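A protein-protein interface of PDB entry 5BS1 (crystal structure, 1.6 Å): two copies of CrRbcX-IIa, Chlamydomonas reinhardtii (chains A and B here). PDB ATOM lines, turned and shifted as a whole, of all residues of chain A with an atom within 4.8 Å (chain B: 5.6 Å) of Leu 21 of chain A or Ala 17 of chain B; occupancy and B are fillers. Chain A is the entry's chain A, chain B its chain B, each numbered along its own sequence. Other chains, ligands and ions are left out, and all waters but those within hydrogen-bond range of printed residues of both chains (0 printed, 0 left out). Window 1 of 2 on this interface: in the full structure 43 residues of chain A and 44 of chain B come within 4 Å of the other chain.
Ala 18 of chain A touches Thr 102 of chain B, and with the chains exchanged Thr 102 of chain A touches Ala 18 of chain B. Leu 21 of chain A touches Trp 99 of chain B, but with the chains exchanged Trp 99 of chain A does not touch Leu 21 of chain B (6.9 Å). Trp 99 of chain B touches its own counterpart, Trp 99 of chain A. Thr 102 of chain A touches Trp 99 of chain B, but with the chains exchanged Trp 99 of chain A does not touch Thr 102 of chain B (4.8 Å). Positions printed for both chains: 17, 18, 19, 20, 21, 22, 99 and 102. Of the 18 pairs that touch across the chains among the printed residues, 5 have their exchanged pair printed and touching as well.
OG of Ser 12 of chain B sits close to N of Glu 14 of chain B (3.5 Å).
Of the 13 printed residues of chain A, 9 touch a printed residue of chain B. Printed residues of chain A that touch a printed residue of chain B: Met 1, Ala 17, Ala 18, Leu 21, Arg 22, Leu 24, Phe 97, Trp 99 and Thr 102. Hydrophobic or aromatic side chains of chain A that line the printed part of chain B: Met 1, Ala 17, Ala 18, Leu 21, Leu 24, Phe 97 and Trp 99. Of the 14 printed residues of chain B, 9 touch a printed residue of chain A. Printed residues of chain B that touch a printed residue of chain A: Pro 13, Glu 14, Lys 16, Ala 17, Ala 18, Ala 20, Trp 99, Thr 102 and Ala 106. Hydrophobic or aromatic side chains of chain B that line the printed part of chain A: Ala 17, Ala 18, Ala 20, Trp 99 and Ala 106. Among the printed residues, 18 pairs touch across the chains. Among the printed residues, no Asp or Glu carboxylate lies within 4 Å of a Lys or Arg side-chain nitrogen of the other chain.
Of the printed residues of chain B, Ala 17 of chain A touches Thr 102 (3.8 Å). Of chain B, only Ala 17 (3.8 Å), Trp 99 (3.8 Å) and Thr 102 (3.7 Å) come within 4 Å of Leu 21 of chain A. Printed residues of chain A within 4 Å of Pro 13 of chain B: Leu 24 (3.8 Å). Of the printed residues of chain A, Ala 17 of chain B touches Leu 21 (3.8 Å), Phe 97 (3.98 Å) and Thr 102 (3.7 Å). Of the printed residues of chain A, Ala 18 of chain B touches Thr 102. Val 19 of chain B touches none of the printed residues of chain A. Printed residues of chain A within 4 Å of Thr 102 of chain B: Ala 17, Ala 18 and Leu 21. Printed residues of chain A within 4 Å of Ala 106 of chain B: Ala 18, Arg 22 and Trp 99.
The backbone carbonyl oxygen (O) of Trp 99 of chain A lies within hydrogen-bond range of the indole nitrogen (NE1) of Trp 99 of chain B, 3.0 Å away.
CB of Ala 20 of chain B touches CG of Met 1 of chain A, 3.9 Å away. Ala 106 of chain B touches Ala 18 of chain A (N to CB, 3.8 Å). Ala 17 of chain B touches Leu 21 of chain A. Thr 102 of chain B touches Leu 21 of chain A. O of Ala 106 of chain B touches CD of Arg 22 of chain A, at 3.5 Å. Pro 13 of chain B touches Leu 24 of chain A (O to CD2, 3.8 Å). Phe 97 of chain A touches Ala 17 of chain B. CH2 of Trp 99 of chain A touches CB of Ala 106 of chain B, at 3.98 Å. Ala 18 of chain B touches Thr 102 of chain A. CH2 of Trp 99 of chain B touches CG2 of Thr 102 of chain A, at 3.97 Å.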
ATOM      1  N   MET A   1      -0.929  -9.768 -35.337  1.00  0.00           N
ATOM      2  CA  MET A   1      -0.984  -9.303 -33.938  1.00  0.00           C
ATOM      3  C   MET A   1      -2.135 -10.017 -33.307  1.00  0.00           C
ATOM      4  O   MET A   1      -3.299  -9.634 -33.464  1.00  0.00           O
ATOM      5  CB  MET A   1      -1.080  -7.780 -33.927  1.00  0.00           C
ATOM      6  CG  MET A   1      -1.157  -7.187 -32.530  1.00  0.00           C
ATOM      7  SD  MET A   1      -1.146  -5.233 -32.781  1.00  0.00           S
ATOM      8  CE  MET A   1      -0.896  -4.620 -30.953  1.00  0.00           C
ATOM      9  N   ALA A  17      -1.145  -7.450 -24.043  1.00  0.00           N
ATOM     10  CA  ALA A  17      -1.324  -6.307 -24.923  1.00  0.00           C
ATOM     11  C   ALA A  17      -0.060  -5.457 -24.958  1.00  0.00           C
ATOM     12  O   ALA A  17       0.347  -5.026 -26.030  1.00  0.00           O
ATOM     13  CB  ALA A  17      -2.530  -5.493 -24.505  1.00  0.00           C
ATOM     14  N   ALA A  18       0.556  -5.244 -23.809  1.00  0.00           N
ATOM     15  CA  ALA A  18       1.791  -4.419 -23.730  1.00  0.00           C
ATOM     16  C   ALA A  18       2.900  -5.046 -24.561  1.00  0.00           C
ATOM     17  O   ALA A  18       3.564  -4.363 -25.326  1.00  0.00           O
ATOM     18  CB  ALA A  18       2.209  -4.238 -22.279  1.00  0.00           C
ATOM     19  N   VAL A  19       3.086  -6.345 -24.432  1.00  0.00           N
ATOM     20  CA  VAL A  19       4.154  -7.041 -25.195  1.00  0.00           C
ATOM     21  C   VAL A  19       3.857  -7.045 -26.693  1.00  0.00           C
ATOM     22  O   VAL A  19       4.731  -6.827 -27.523  1.00  0.00           O
ATOM     23  CB  VAL A  19       4.400  -8.448 -24.626  1.00  0.00           C
ATOM     24  CG1 VAL A  19       5.408  -9.184 -25.469  1.00  0.00           C
ATOM     25  CG2 VAL A  19       4.885  -8.309 -23.190  1.00  0.00           C
ATOM     26  N   ALA A  20       2.589  -7.241 -27.043  1.00  0.00           N
ATOM     27  CA  ALA A  20       2.167  -7.172 -28.440  1.00  0.00           C
ATOM     28  C   ALA A  20       2.429  -5.777 -29.004  1.00  0.00           C
ATOM     29  O   ALA A  20       2.896  -5.627 -30.140  1.00  0.00           O
ATOM     30  CB  ALA A  20       0.702  -7.514 -28.553  1.00  0.00           C
ATOM     31  N   LEU A  21       2.126  -4.752 -28.224  1.00  0.00           N
ATOM     32  CA  LEU A  21       2.384  -3.357 -28.654  1.00  0.00           C
ATOM     33  C   LEU A  21       3.882  -3.133 -28.844  1.00  0.00           C
ATOM     34  O   LEU A  21       4.298  -2.495 -29.813  1.00  0.00           O
ATOM     35  CB  LEU A  21       1.838  -2.327 -27.667  1.00  0.00           C
ATOM     36  CG  LEU A  21       0.322  -2.152 -27.661  1.00  0.00           C
ATOM     37  CD1 LEU A  21      -0.077  -1.354 -26.458  1.00  0.00           C
ATOM     38  CD2 LEU A  21      -0.187  -1.522 -28.940  1.00  0.00           C
ATOM     39  N   ARG A  22       4.698  -3.684 -27.951  1.00  0.00           N
ATOM     40  CA  ARG A  22       6.143  -3.540 -28.087  1.00  0.00           C
ATOM     41  C   ARG A  22       6.617  -4.101 -29.407  1.00  0.00           C
ATOM     42  O   ARG A  22       7.477  -3.506 -30.072  1.00  0.00           O
ATOM     43  CB  ARG A  22       6.860  -4.210 -26.895  1.00  0.00           C
ATOM     44  CG  ARG A  22       6.700  -3.406 -25.589  1.00  0.00           C
ATOM     45  CD  ARG A  22       7.802  -3.656 -24.576  1.00  0.00           C
ATOM     46  NE  ARG A  22       9.042  -3.369 -25.262  1.00  0.00           N
ATOM     47  CZ  ARG A  22      10.069  -4.186 -25.445  1.00  0.00           C
ATOM     48  NH1 ARG A  22      11.026  -3.792 -26.283  1.00  0.00           N
ATOM     49  NH2 ARG A  22      10.189  -5.329 -24.768  1.00  0.00           N
ATOM     50  N   SER A  23       6.098  -5.263 -29.788  1.00  0.00           N
ATOM     51  CA  SER A  23       6.454  -5.865 -31.092  1.00  0.00           C
ATOM     52  C   SER A  23       5.966  -5.000 -32.233  1.00  0.00           C
ATOM     53  O   SER A  23       6.673  -4.764 -33.227  1.00  0.00           O
ATOM     54  CB  SER A  23       5.901  -7.276 -31.267  1.00  0.00           C
ATOM     55  OG  SER A  23       6.568  -8.182 -30.426  1.00  0.00           O
ATOM     56  N   LEU A  24       4.741  -4.494 -32.113  1.00  0.00           N
ATOM     57  CA  LEU A  24       4.215  -3.566 -33.121  1.00  0.00           C
ATOM     58  C   LEU A  24       5.121  -2.339 -33.289  1.00  0.00           C
ATOM     59  O   LEU A  24       5.431  -1.916 -34.407  1.00  0.00           O
ATOM     60  CB  LEU A  24       2.792  -3.141 -32.761  1.00  0.00           C
ATOM     61  CG  LEU A  24       2.155  -2.098 -33.677  1.00  0.00           C
ATOM     62  CD1 LEU A  24       1.991  -2.624 -35.091  1.00  0.00           C
ATOM     63  CD2 LEU A  24       0.834  -1.583 -33.133  1.00  0.00           C
ATOM     64  N   PHE A  25       5.572  -1.757 -32.187  1.00  0.00           N
ATOM     65  CA  PHE A  25       6.398  -0.565 -32.215  1.00  0.00           C
ATOM     66  C   PHE A  25       7.747  -0.845 -32.853  1.00  0.00           C
ATOM     67  O   PHE A  25       8.289  -0.007 -33.570  1.00  0.00           O
ATOM     68  CB  PHE A  25       6.546   0.049 -30.821  1.00  0.00           C
ATOM     69  CG  PHE A  25       5.234   0.460 -30.153  1.00  0.00           C
ATOM     70  CD1 PHE A  25       4.052   0.676 -30.867  1.00  0.00           C
ATOM     71  CD2 PHE A  25       5.229   0.695 -28.799  1.00  0.00           C
ATOM     72  CE1 PHE A  25       2.877   1.064 -30.217  1.00  0.00           C
ATOM     73  CE2 PHE A  25       4.061   1.065 -28.150  1.00  0.00           C
ATOM     74  CZ  PHE A  25       2.893   1.274 -28.862  1.00  0.00           C
ATOM     75  N   PHE A  97       2.661   7.589 -30.457  1.00  0.00           N
ATOM     76  CA  PHE A  97       1.496   6.700 -30.554  1.00  0.00           C
ATOM     77  C   PHE A  97       0.327   7.311 -29.800  1.00  0.00           C
ATOM     78  O   PHE A  97       0.463   7.797 -28.680  1.00  0.00           O
ATOM     79  CB  PHE A  97       1.847   5.336 -29.962  1.00  0.00           C
ATOM     80  CG  PHE A  97       0.787   4.278 -30.106  1.00  0.00           C
ATOM     81  CD1 PHE A  97       0.514   3.696 -31.338  1.00  0.00           C
ATOM     82  CD2 PHE A  97       0.106   3.797 -29.000  1.00  0.00           C
ATOM     83  CE1 PHE A  97      -0.404   2.692 -31.460  1.00  0.00           C
ATOM     84  CE2 PHE A  97      -0.823   2.809 -29.120  1.00  0.00           C
ATOM     85  CZ  PHE A  97      -1.108   2.257 -30.358  1.00  0.00           C
ATOM     86  N   TRP A  99      -2.315   6.846 -27.736  1.00  0.00           N
ATOM     87  CA  TRP A  99      -2.796   5.870 -26.768  1.00  0.00           C
ATOM     88  C   TRP A  99      -4.268   6.014 -26.497  1.00  0.00           C
ATOM     89  O   TRP A  99      -4.997   5.028 -26.501  1.00  0.00           O
ATOM     90  CB  TRP A  99      -2.036   6.035 -25.431  1.00  0.00           C
ATOM     91  CG  TRP A  99      -0.590   5.720 -25.550  1.00  0.00           C
ATOM     92  CD1 TRP A  99       0.435   6.609 -25.768  1.00  0.00           C
ATOM     93  CD2 TRP A  99       0.014   4.426 -25.458  1.00  0.00           C
ATOM     94  NE1 TRP A  99       1.621   5.935 -25.855  1.00  0.00           N
ATOM     95  CE2 TRP A  99       1.406   4.603 -25.633  1.00  0.00           C
ATOM     96  CE3 TRP A  99      -0.479   3.150 -25.240  1.00  0.00           C
ATOM     97  CZ2 TRP A  99       2.293   3.539 -25.619  1.00  0.00           C
ATOM     98  CZ3 TRP A  99       0.421   2.073 -25.229  1.00  0.00           C
ATOM     99  CH2 TRP A  99       1.780   2.289 -25.405  1.00  0.00           C
ATOM    100  N   THR A 102      -6.531   4.986 -29.417  1.00  0.00           N
ATOM    101  CA  THR A 102      -6.545   3.560 -29.636  1.00  0.00           C
ATOM    102  C   THR A 102      -7.585   2.858 -28.756  1.00  0.00           C
ATOM    103  O   THR A 102      -8.384   2.044 -29.238  1.00  0.00           O
ATOM    104  CB  THR A 102      -5.135   2.986 -29.373  1.00  0.00           C
ATOM    105  OG1 THR A 102      -4.221   3.579 -30.283  1.00  0.00           O
ATOM    106  CG2 THR A 102      -5.101   1.471 -29.574  1.00  0.00           C
ATOM    107  N   SER B  12      -3.773   2.743 -39.699  1.00  0.00           N
ATOM    108  CA  SER B  12      -2.705   3.243 -38.841  1.00  0.00           C
ATOM    109  C   SER B  12      -2.330   2.168 -37.820  1.00  0.00           C
ATOM    110  O   SER B  12      -3.100   1.244 -37.599  1.00  0.00           O
ATOM    111  CB  SER B  12      -3.190   4.442 -38.069  1.00  0.00           C
ATOM    112  OG  SER B  12      -4.304   4.066 -37.263  1.00  0.00           O
ATOM    113  N   PRO B  13      -1.159   2.300 -37.187  1.00  0.00           N
ATOM    114  CA  PRO B  13      -0.850   1.366 -36.099  1.00  0.00           C
ATOM    115  C   PRO B  13      -1.890   1.431 -34.978  1.00  0.00           C
ATOM    116  O   PRO B  13      -2.180   0.424 -34.364  1.00  0.00           O
ATOM    117  CB  PRO B  13       0.530   1.845 -35.629  1.00  0.00           C
ATOM    118  CG  PRO B  13       1.129   2.398 -36.873  1.00  0.00           C
ATOM    119  CD  PRO B  13      -0.002   3.142 -37.522  1.00  0.00           C
ATOM    120  N   GLU B  14      -2.427   2.621 -34.702  1.00  0.00           N
ATOM    121  CA  GLU B  14      -3.488   2.761 -33.727  1.00  0.00           C
ATOM    122  C   GLU B  14      -4.719   1.933 -34.078  1.00  0.00           C
ATOM    123  O   GLU B  14      -5.281   1.266 -33.204  1.00  0.00           O
ATOM    124  CB  GLU B  14      -3.873   4.228 -33.551  1.00  0.00           C
ATOM    125  CG  GLU B  14      -2.826   5.034 -32.817  1.00  0.00           C
ATOM    126  CD  GLU B  14      -1.774   5.681 -33.711  1.00  0.00           C
ATOM    127  OE1 GLU B  14      -1.736   5.420 -34.941  1.00  0.00           O
ATOM    128  OE2 GLU B  14      -0.963   6.477 -33.162  1.00  0.00           O
ATOM    129  N   ARG B  15      -5.118   1.957 -35.351  1.00  0.00           N
ATOM    130  CA  ARG B  15      -6.246   1.129 -35.781  1.00  0.00           C
ATOM    131  C   ARG B  15      -5.902  -0.355 -35.647  1.00  0.00           C
ATOM    132  O   ARG B  15      -6.720  -1.147 -35.216  1.00  0.00           O
ATOM    133  CB  ARG B  15      -6.711   1.465 -37.188  1.00  0.00           C
ATOM    134  CG  ARG B  15      -7.784   0.487 -37.622  1.00  0.00           C
ATOM    135  CD  ARG B  15      -8.658   1.016 -38.706  1.00  0.00           C
ATOM    136  NE  ARG B  15      -9.517   2.052 -38.177  1.00  0.00           N
ATOM    137  CZ  ARG B  15     -10.630   1.837 -37.466  1.00  0.00           C
ATOM    138  NH1 ARG B  15     -11.053   0.604 -37.199  1.00  0.00           N
ATOM    139  NH2 ARG B  15     -11.300   2.877 -37.001  1.00  0.00           N
ATOM    140  N   LYS B  16      -4.689  -0.734 -36.061  1.00  0.00           N
ATOM    141  CA  LYS B  16      -4.269  -2.124 -35.939  1.00  0.00           C
ATOM    142  C   LYS B  16      -4.363  -2.600 -34.486  1.00  0.00           C
ATOM    143  O   LYS B  16      -4.940  -3.680 -34.168  1.00  0.00           O
ATOM    144  CB  LYS B  16      -2.843  -2.288 -36.513  1.00  0.00           C
ATOM    145  CG  LYS B  16      -2.274  -3.711 -36.413  1.00  0.00           C
ATOM    146  CD  LYS B  16      -3.078  -4.683 -37.224  1.00  0.00           C
ATOM    147  CE  LYS B  16      -2.599  -6.122 -37.030  1.00  0.00           C
ATOM    148  NZ  LYS B  16      -3.571  -7.058 -37.627  1.00  0.00           N
ATOM    149  N   ALA B  17      -3.845  -1.783 -33.587  1.00  0.00           N
ATOM    150  CA  ALA B  17      -3.878  -2.069 -32.181  1.00  0.00           C
ATOM    151  C   ALA B  17      -5.299  -2.132 -31.638  1.00  0.00           C
ATOM    152  O   ALA B  17      -5.625  -3.022 -30.834  1.00  0.00           O
ATOM    153  CB  ALA B  17      -3.068  -1.044 -31.415  1.00  0.00           C
ATOM    154  N   ALA B  18      -6.129  -1.200 -32.073  1.00  0.00           N
ATOM    155  CA  ALA B  18      -7.529  -1.151 -31.633  1.00  0.00           C
ATOM    156  C   ALA B  18      -8.287  -2.413 -31.999  1.00  0.00           C
ATOM    157  O   ALA B  18      -8.988  -2.989 -31.178  1.00  0.00           O
ATOM    158  CB  ALA B  18      -8.234   0.083 -32.192  1.00  0.00           C
ATOM    159  N   VAL B  19      -8.113  -2.875 -33.234  1.00  0.00           N
ATOM    160  CA  VAL B  19      -8.782  -4.107 -33.660  1.00  0.00           C
ATOM    161  C   VAL B  19      -8.237  -5.335 -32.919  1.00  0.00           C
ATOM    162  O   VAL B  19      -8.997  -6.223 -32.531  1.00  0.00           O
ATOM    163  CB  VAL B  19      -8.719  -4.255 -35.184  1.00  0.00           C
ATOM    164  CG1 VAL B  19      -9.347  -5.577 -35.626  1.00  0.00           C
ATOM    165  CG2 VAL B  19      -9.434  -3.069 -35.837  1.00  0.00           C
ATOM    166  N   ALA B  20      -6.938  -5.360 -32.682  1.00  0.00           N
ATOM    167  CA  ALA B  20      -6.328  -6.412 -31.881  1.00  0.00           C
ATOM    168  C   ALA B  20      -6.877  -6.418 -30.459  1.00  0.00           C
ATOM    169  O   ALA B  20      -7.173  -7.484 -29.925  1.00  0.00           O
ATOM    170  CB  ALA B  20      -4.831  -6.247 -31.866  1.00  0.00           C
ATOM    171  N   LEU B  21      -7.079  -5.232 -29.874  1.00  0.00           N
ATOM    172  CA  LEU B  21      -7.685  -5.136 -28.547  1.00  0.00           C
ATOM    173  C   LEU B  21      -9.108  -5.698 -28.552  1.00  0.00           C
ATOM    174  O   LEU B  21      -9.511  -6.417 -27.644  1.00  0.00           O
ATOM    175  CB  LEU B  21      -7.693  -3.700 -28.023  1.00  0.00           C
ATOM    176  CG  LEU B  21      -6.339  -3.169 -27.561  1.00  0.00           C
ATOM    177  CD1 LEU B  21      -6.483  -1.677 -27.319  1.00  0.00           C
ATOM    178  CD2 LEU B  21      -5.836  -3.854 -26.319  1.00  0.00           C
ATOM    179  N   ARG B  22      -9.852  -5.365 -29.580  1.00  0.00           N
ATOM    180  CA  ARG B  22     -11.249  -5.821 -29.699  1.00  0.00           C
ATOM    181  C   ARG B  22     -11.311  -7.349 -29.732  1.00  0.00           C
ATOM    182  O   ARG B  22     -12.137  -7.970 -29.047  1.00  0.00           O
ATOM    183  CB  ARG B  22     -11.889  -5.232 -30.924  1.00  0.00           C
ATOM    184  CG  ARG B  22     -12.161  -3.748 -30.821  1.00  0.00           C
ATOM    185  CD  ARG B  22     -13.306  -3.314 -31.686  1.00  0.00           C
ATOM    186  NE  ARG B  22     -14.375  -4.216 -31.318  1.00  0.00           N
ATOM    187  CZ  ARG B  22     -15.128  -4.943 -32.141  1.00  0.00           C
ATOM    188  NH1 ARG B  22     -15.992  -5.792 -31.588  1.00  0.00           N
ATOM    189  NH2 ARG B  22     -15.031  -4.826 -33.465  1.00  0.00           N
ATOM    190  N   TRP B  99      -5.921  -0.247 -19.397  1.00  0.00           N
ATOM    191  CA  TRP B  99      -5.159   0.236 -20.535  1.00  0.00           C
ATOM    192  C   TRP B  99      -4.007   1.124 -20.092  1.00  0.00           C
ATOM    193  O   TRP B  99      -2.961   1.111 -20.749  1.00  0.00           O
ATOM    194  CB  TRP B  99      -6.083   0.956 -21.489  1.00  0.00           C
ATOM    195  CG  TRP B  99      -5.457   1.643 -22.685  1.00  0.00           C
ATOM    196  CD1 TRP B  99      -5.518   2.971 -22.953  1.00  0.00           C
ATOM    197  CD2 TRP B  99      -4.731   1.046 -23.773  1.00  0.00           C
ATOM    198  NE1 TRP B  99      -4.899   3.239 -24.129  1.00  0.00           N
ATOM    199  CE2 TRP B  99      -4.393   2.078 -24.651  1.00  0.00           C
ATOM    200  CE3 TRP B  99      -4.336  -0.255 -24.092  1.00  0.00           C
ATOM    201  CZ2 TRP B  99      -3.709   1.852 -25.828  1.00  0.00           C
ATOM    202  CZ3 TRP B  99      -3.628  -0.484 -25.263  1.00  0.00           C
ATOM    203  CH2 TRP B  99      -3.337   0.568 -26.129  1.00  0.00           C
ATOM    204  N   THR B 102      -1.173  -1.149 -19.385  1.00  0.00           N
ATOM    205  CA  THR B 102      -0.624  -1.601 -20.637  1.00  0.00           C
ATOM    206  C   THR B 102       0.358  -0.570 -21.187  1.00  0.00           C
ATOM    207  O   THR B 102       1.459  -0.908 -21.583  1.00  0.00           O
ATOM    208  CB  THR B 102      -1.724  -1.886 -21.663  1.00  0.00           C
ATOM    209  OG1 THR B 102      -2.513  -2.992 -21.196  1.00  0.00           O
ATOM    210  CG2 THR B 102      -1.162  -2.223 -23.012  1.00  0.00           C
ATOM    211  N   ALA B 106       4.334  -1.197 -21.626  1.00  0.00           N
ATOM    212  CA  ALA B 106       4.898  -1.159 -22.985  1.00  0.00           C
ATOM    213  C   ALA B 106       6.017  -0.126 -23.024  1.00  0.00           C
ATOM    214  O   ALA B 106       7.079  -0.384 -23.643  1.00  0.00           O
ATOM    215  CB  ALA B 106       3.838  -0.831 -24.023  1.00  0.00           C
